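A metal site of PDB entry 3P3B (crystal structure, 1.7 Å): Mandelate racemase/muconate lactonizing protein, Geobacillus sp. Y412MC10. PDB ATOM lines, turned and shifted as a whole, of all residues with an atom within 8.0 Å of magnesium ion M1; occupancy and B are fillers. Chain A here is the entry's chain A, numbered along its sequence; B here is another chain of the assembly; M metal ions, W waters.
Magnesium ion M1 is bound by OD1 of Asp 261 (2.1 Å), water W1 (2.1 Å), OE2 of Glu 234 (2.1 Å), OE2 of Glu 238 (2.2 Å), water W3 (2.2 Å) and water W2 (2.2 Å). Magnesium ion M1 has six donor atoms within binding distance.
Of the 21 residues printed, 3 come within 4 Å of magnesium ion M1.
OD2 of Asp 261 is in hydrogen-bond range of OH of Tyr 243. N of Gln 283 is in hydrogen-bond range of O of Asp 261. The backbone carbonyl oxygen (O) of Glu 234 is in hydrogen-bond range of the backbone NH (N) of Asn 210, at 2.8 Å. N of Glu 234 lies within hydrogen-bond range of O of Ala 260 (3.1 Å). The backbone NH (N) of Asn 209 sits at hydrogen-bond distance from the backbone carbonyl oxygen (O) of Glu 234, 3.4 Å away. The side-chain carboxylate (OE2) of Glu 238 lies close to a ring nitrogen (ND1) of His 237 of chain A (3.5 Å). The side-chain carboxylate of Glu 238 is in hydrogen-bond range of the backbone NH of Ser 267, 2.9 Å away.
Water W2 lies within hydrogen-bond range of ND1 of His 237 of chain A (2.7 Å) and ND2 of Asn 210 (2.9 Å). Water W3 lies within hydrogen-bond range of O of Glu 263, OE1 of Glu 238 and N of Gly 262.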
ATOM      1  N   ASN A 209     -11.096 -21.500 -28.234  1.00  0.00           N
ATOM      2  CA  ASN A 209     -11.044 -20.274 -27.436  1.00  0.00           C
ATOM      3  C   ASN A 209     -10.516 -20.484 -26.012  1.00  0.00           C
ATOM      4  O   ASN A 209     -11.088 -20.008 -25.031  1.00  0.00           O
ATOM      5  CB  ASN A 209     -12.396 -19.536 -27.465  1.00  0.00           C
ATOM      6  CG  ASN A 209     -12.716 -18.997 -28.836  1.00  0.00           C
ATOM      7  OD1 ASN A 209     -13.439 -19.622 -29.601  1.00  0.00           O
ATOM      8  ND2 ASN A 209     -12.136 -17.848 -29.172  1.00  0.00           N
ATOM      9  N   ASN A 210      -9.420 -21.241 -25.949  1.00  0.00           N
ATOM     10  CA  ASN A 210      -8.658 -21.527 -24.736  1.00  0.00           C
ATOM     11  C   ASN A 210      -9.348 -22.382 -23.672  1.00  0.00           C
ATOM     12  O   ASN A 210      -8.848 -22.473 -22.558  1.00  0.00           O
ATOM     13  CB  ASN A 210      -8.090 -20.239 -24.125  1.00  0.00           C
ATOM     14  CG  ASN A 210      -6.961 -19.667 -24.959  1.00  0.00           C
ATOM     15  OD1 ASN A 210      -6.317 -20.388 -25.736  1.00  0.00           O
ATOM     16  ND2 ASN A 210      -6.693 -18.366 -24.805  1.00  0.00           N
ATOM     17  N   GLU A 233      -6.901 -24.379 -33.232  1.00  0.00           N
ATOM     18  CA  GLU A 233      -6.693 -22.977 -32.881  1.00  0.00           C
ATOM     19  C   GLU A 233      -7.014 -22.719 -31.418  1.00  0.00           C
ATOM     20  O   GLU A 233      -8.093 -23.101 -30.933  1.00  0.00           O
ATOM     21  CB  GLU A 233      -7.549 -22.103 -33.804  1.00  0.00           C
ATOM     22  CG  GLU A 233      -7.646 -20.640 -33.381  1.00  0.00           C
ATOM     23  CD  GLU A 233      -8.261 -19.774 -34.456  1.00  0.00           C
ATOM     24  OE1 GLU A 233      -8.371 -20.210 -35.630  1.00  0.00           O
ATOM     25  OE2 GLU A 233      -8.605 -18.626 -34.144  1.00  0.00           O
ATOM     26  N   GLU A 234      -6.081 -22.074 -30.717  1.00  0.00           N
ATOM     27  CA  GLU A 234      -6.258 -21.720 -29.293  1.00  0.00           C
ATOM     28  C   GLU A 234      -6.855 -22.845 -28.450  1.00  0.00           C
ATOM     29  O   GLU A 234      -7.894 -22.698 -27.802  1.00  0.00           O
ATOM     30  CB  GLU A 234      -7.066 -20.426 -29.163  1.00  0.00           C
ATOM     31  CG  GLU A 234      -6.332 -19.206 -29.747  1.00  0.00           C
ATOM     32  CD  GLU A 234      -6.697 -17.896 -29.042  1.00  0.00           C
ATOM     33  OE1 GLU A 234      -7.876 -17.479 -29.086  1.00  0.00           O
ATOM     34  OE2 GLU A 234      -5.773 -17.275 -28.475  1.00  0.00           O
ATOM     35  N   ALA A 235      -6.184 -23.989 -28.430  1.00  0.00           N
ATOM     36  CA  ALA A 235      -6.670 -25.111 -27.624  1.00  0.00           C
ATOM     37  C   ALA A 235      -6.661 -24.683 -26.163  1.00  0.00           C
ATOM     38  O   ALA A 235      -7.575 -24.974 -25.401  1.00  0.00           O
ATOM     39  CB  ALA A 235      -5.778 -26.354 -27.838  1.00  0.00           C
ATOM     40  N   PHE A 236      -5.607 -23.956 -25.796  1.00  0.00           N
ATOM     41  CA  PHE A 236      -5.431 -23.377 -24.475  1.00  0.00           C
ATOM     42  C   PHE A 236      -4.473 -22.211 -24.670  1.00  0.00           C
ATOM     43  O   PHE A 236      -3.859 -22.091 -25.722  1.00  0.00           O
ATOM     44  CB  PHE A 236      -4.761 -24.385 -23.530  1.00  0.00           C
ATOM     45  CG  PHE A 236      -3.749 -25.254 -24.208  1.00  0.00           C
ATOM     46  CD1 PHE A 236      -4.063 -26.553 -24.587  1.00  0.00           C
ATOM     47  CD2 PHE A 236      -2.475 -24.770 -24.471  1.00  0.00           C
ATOM     48  CE1 PHE A 236      -3.143 -27.370 -25.216  1.00  0.00           C
ATOM     49  CE2 PHE A 236      -1.533 -25.599 -25.118  1.00  0.00           C
ATOM     50  CZ  PHE A 236      -1.869 -26.887 -25.480  1.00  0.00           C
ATOM     51  N   HIS A 237      -4.343 -21.367 -23.665  1.00  0.00           N
ATOM     52  CA  HIS A 237      -3.473 -20.226 -23.831  1.00  0.00           C
ATOM     53  C   HIS A 237      -2.062 -20.702 -24.153  1.00  0.00           C
ATOM     54  O   HIS A 237      -1.525 -21.596 -23.473  1.00  0.00           O
ATOM     55  CB  HIS A 237      -3.452 -19.346 -22.585  1.00  0.00           C
ATOM     56  CG  HIS A 237      -2.614 -18.124 -22.749  1.00  0.00           C
ATOM     57  ND1 HIS A 237      -2.917 -17.132 -23.639  1.00  0.00           N
ATOM     58  CD2 HIS A 237      -1.453 -17.769 -22.155  1.00  0.00           C
ATOM     59  CE1 HIS A 237      -1.991 -16.188 -23.579  1.00  0.00           C
ATOM     60  NE2 HIS A 237      -1.097 -16.553 -22.681  1.00  0.00           N
ATOM     61  N   GLU A 238      -1.476 -20.110 -25.179  1.00  0.00           N
ATOM     62  CA  GLU A 238      -0.179 -20.535 -25.707  1.00  0.00           C
ATOM     63  C   GLU A 238       0.885 -20.725 -24.627  1.00  0.00           C
ATOM     64  O   GLU A 238       1.063 -19.890 -23.731  1.00  0.00           O
ATOM     65  CB  GLU A 238       0.324 -19.612 -26.826  1.00  0.00           C
ATOM     66  CG  GLU A 238       0.460 -18.145 -26.461  1.00  0.00           C
ATOM     67  CD  GLU A 238      -0.776 -17.351 -26.875  1.00  0.00           C
ATOM     68  OE1 GLU A 238      -0.639 -16.172 -27.248  1.00  0.00           O
ATOM     69  OE2 GLU A 238      -1.869 -17.926 -26.839  1.00  0.00           O
ATOM     70  N   ASP A 239       1.588 -21.855 -24.725  1.00  0.00           N
ATOM     71  CA  ASP A 239       2.551 -22.299 -23.731  1.00  0.00           C
ATOM     72  C   ASP A 239       3.554 -23.164 -24.500  1.00  0.00           C
ATOM     73  O   ASP A 239       3.160 -24.155 -25.113  1.00  0.00           O
ATOM     74  CB  ASP A 239       1.822 -23.119 -22.658  1.00  0.00           C
ATOM     75  CG  ASP A 239       2.740 -23.616 -21.535  1.00  0.00           C
ATOM     76  OD1 ASP A 239       3.885 -24.043 -21.801  1.00  0.00           O
ATOM     77  OD2 ASP A 239       2.295 -23.593 -20.359  1.00  0.00           O
ATOM     78  N   TYR A 243       2.766 -26.932 -26.033  1.00  0.00           N
ATOM     79  CA  TYR A 243       2.751 -27.072 -27.488  1.00  0.00           C
ATOM     80  C   TYR A 243       3.859 -28.014 -27.989  1.00  0.00           C
ATOM     81  O   TYR A 243       3.650 -28.773 -28.935  1.00  0.00           O
ATOM     82  CB  TYR A 243       2.810 -25.697 -28.146  1.00  0.00           C
ATOM     83  CG  TYR A 243       1.431 -25.020 -28.342  1.00  0.00           C
ATOM     84  CD1 TYR A 243       0.267 -25.781 -28.520  1.00  0.00           C
ATOM     85  CD2 TYR A 243       1.331 -23.649 -28.403  1.00  0.00           C
ATOM     86  CE1 TYR A 243      -0.986 -25.143 -28.723  1.00  0.00           C
ATOM     87  CE2 TYR A 243       0.101 -23.018 -28.611  1.00  0.00           C
ATOM     88  CZ  TYR A 243      -1.046 -23.761 -28.773  1.00  0.00           C
ATOM     89  OH  TYR A 243      -2.240 -23.108 -28.988  1.00  0.00           O
ATOM     90  N   ALA A 260      -2.399 -23.412 -34.479  1.00  0.00           N
ATOM     91  CA  ALA A 260      -2.659 -21.993 -34.789  1.00  0.00           C
ATOM     92  C   ALA A 260      -2.930 -21.182 -33.508  1.00  0.00           C
ATOM     93  O   ALA A 260      -3.630 -21.644 -32.610  1.00  0.00           O
ATOM     94  CB  ALA A 260      -3.874 -21.888 -35.736  1.00  0.00           C
ATOM     95  N   ASP A 261      -2.354 -19.995 -33.416  1.00  0.00           N
ATOM     96  CA  ASP A 261      -2.530 -19.161 -32.232  1.00  0.00           C
ATOM     97  C   ASP A 261      -2.140 -17.714 -32.583  1.00  0.00           C
ATOM     98  O   ASP A 261      -1.606 -17.457 -33.659  1.00  0.00           O
ATOM     99  CB  ASP A 261      -1.702 -19.710 -31.047  1.00  0.00           C
ATOM    100  CG  ASP A 261      -2.445 -19.554 -29.726  1.00  0.00           C
ATOM    101  OD1 ASP A 261      -3.096 -18.497 -29.558  1.00  0.00           O
ATOM    102  OD2 ASP A 261      -2.410 -20.472 -28.871  1.00  0.00           O
ATOM    103  N   GLY A 262      -2.433 -16.794 -31.668  1.00  0.00           N
ATOM    104  CA  GLY A 262      -1.925 -15.434 -31.786  1.00  0.00           C
ATOM    105  C   GLY A 262      -2.957 -14.314 -31.726  1.00  0.00           C
ATOM    106  O   GLY A 262      -2.566 -13.143 -31.661  1.00  0.00           O
ATOM    107  N   GLU A 263      -4.247 -14.635 -31.735  1.00  0.00           N
ATOM    108  CA  GLU A 263      -5.219 -13.549 -31.588  1.00  0.00           C
ATOM    109  C   GLU A 263      -5.257 -13.008 -30.144  1.00  0.00           C
ATOM    110  O   GLU A 263      -4.690 -13.596 -29.233  1.00  0.00           O
ATOM    111  CB  GLU A 263      -6.608 -13.999 -32.025  1.00  0.00           C
ATOM    112  CG  GLU A 263      -7.347 -14.787 -30.962  1.00  0.00           C
ATOM    113  CD  GLU A 263      -8.625 -15.402 -31.461  1.00  0.00           C
ATOM    114  OE1 GLU A 263      -9.690 -15.073 -30.890  1.00  0.00           O
ATOM    115  OE2 GLU A 263      -8.569 -16.201 -32.434  1.00  0.00           O
ATOM    116  N   GLY A 264      -5.940 -11.876 -29.950  1.00  0.00           N
ATOM    117  CA  GLY A 264      -6.124 -11.322 -28.625  1.00  0.00           C
ATOM    118  C   GLY A 264      -4.835 -10.881 -27.940  1.00  0.00           C
ATOM    119  O   GLY A 264      -3.893 -10.426 -28.586  1.00  0.00           O
ATOM    120  N   LEU A 265      -4.796 -10.981 -26.626  1.00  0.00           N
ATOM    121  CA  LEU A 265      -3.591 -10.584 -25.882  1.00  0.00           C
ATOM    122  C   LEU A 265      -2.613 -11.749 -25.927  1.00  0.00           C
ATOM    123  O   LEU A 265      -2.652 -12.630 -25.063  1.00  0.00           O
ATOM    124  CB  LEU A 265      -3.937 -10.243 -24.432  1.00  0.00           C
ATOM    125  CG  LEU A 265      -4.911  -9.067 -24.302  1.00  0.00           C
ATOM    126  CD1 LEU A 265      -5.566  -8.986 -22.909  1.00  0.00           C
ATOM    127  CD2 LEU A 265      -4.181  -7.782 -24.660  1.00  0.00           C
ATOM    128  N   ALA A 266      -1.739 -11.757 -26.924  1.00  0.00           N
ATOM    129  CA  ALA A 266      -0.890 -12.940 -27.143  1.00  0.00           C
ATOM    130  C   ALA A 266       0.379 -12.906 -26.288  1.00  0.00           C
ATOM    131  O   ALA A 266       0.826 -11.846 -25.855  1.00  0.00           O
ATOM    132  CB  ALA A 266      -0.559 -13.093 -28.627  1.00  0.00           C
ATOM    133  N   SER A 267       0.945 -14.086 -26.033  1.00  0.00           N
ATOM    134  CA  SER A 267       2.226 -14.152 -25.368  1.00  0.00           C
ATOM    135  C   SER A 267       3.230 -13.379 -26.183  1.00  0.00           C
ATOM    136  O   SER A 267       3.295 -13.546 -27.404  1.00  0.00           O
ATOM    137  CB  SER A 267       2.703 -15.599 -25.247  1.00  0.00           C
ATOM    138  OG  SER A 267       4.083 -15.594 -24.927  1.00  0.00           O
ATOM    139  N   LEU A 270       5.413 -15.564 -28.406  1.00  0.00           N
ATOM    140  CA  LEU A 270       4.775 -16.499 -29.333  1.00  0.00           C
ATOM    141  C   LEU A 270       5.538 -16.737 -30.649  1.00  0.00           C
ATOM    142  O   LEU A 270       5.643 -17.874 -31.117  1.00  0.00           O
ATOM    143  CB  LEU A 270       3.344 -16.030 -29.638  1.00  0.00           C
ATOM    144  CG  LEU A 270       2.587 -16.933 -30.600  1.00  0.00           C
ATOM    145  CD1 LEU A 270       2.443 -18.317 -30.021  1.00  0.00           C
ATOM    146  CD2 LEU A 270       1.174 -16.328 -30.936  1.00  0.00           C
ATOM    147  N   GLN A 283      -1.772 -15.731 -35.892  1.00  0.00           N
ATOM    148  CA  GLN A 283      -3.114 -15.177 -36.127  1.00  0.00           C
ATOM    149  C   GLN A 283      -3.351 -13.779 -35.526  1.00  0.00           C
ATOM    150  O   GLN A 283      -4.447 -13.449 -35.069  1.00  0.00           O
ATOM    151  CB  GLN A 283      -4.165 -16.181 -35.637  1.00  0.00           C
ATOM    152  CG  GLN A 283      -4.096 -17.520 -36.358  1.00  0.00           C
ATOM    153  CD  GLN A 283      -5.159 -18.493 -35.841  1.00  0.00           C
ATOM    154  OE1 GLN A 283      -5.251 -18.752 -34.646  1.00  0.00           O
ATOM    155  NE2 GLN A 283      -5.961 -19.036 -36.755  1.00  0.00           N
ATOM    156  N   HIS B 237      -5.259 -19.731 -17.463  1.00  0.00           N
ATOM    157  CA  HIS B 237      -4.668 -18.431 -17.761  1.00  0.00           C
ATOM    158  C   HIS B 237      -5.683 -17.324 -17.495  1.00  0.00           C
ATOM    159  O   HIS B 237      -6.856 -17.438 -17.918  1.00  0.00           O
ATOM    160  CB  HIS B 237      -4.178 -18.326 -19.198  1.00  0.00           C
ATOM    161  CG  HIS B 237      -3.540 -16.999 -19.497  1.00  0.00           C
ATOM    162  ND1 HIS B 237      -2.331 -16.620 -18.956  1.00  0.00           N
ATOM    163  CD2 HIS B 237      -3.966 -15.951 -20.243  1.00  0.00           C
ATOM    164  CE1 HIS B 237      -2.023 -15.400 -19.386  1.00  0.00           C
ATOM    165  NE2 HIS B 237      -3.004 -14.976 -20.164  1.00  0.00           N
HETATM  166 MG    MG M   1      -3.794 -17.634 -27.769  1.00  0.00          MG
HETATM  167 MG    MG M   2      -9.960 -17.854 -32.801  1.00  0.00          MG
HETATM  168  O   HOH W   1      -4.315 -19.540 -27.037  1.00  0.00           O
HETATM  169  O   HOH W   2      -4.451 -16.803 -25.818  1.00  0.00           O
HETATM  170  O   HOH W   3      -3.109 -15.758 -28.630  1.00  0.00           O
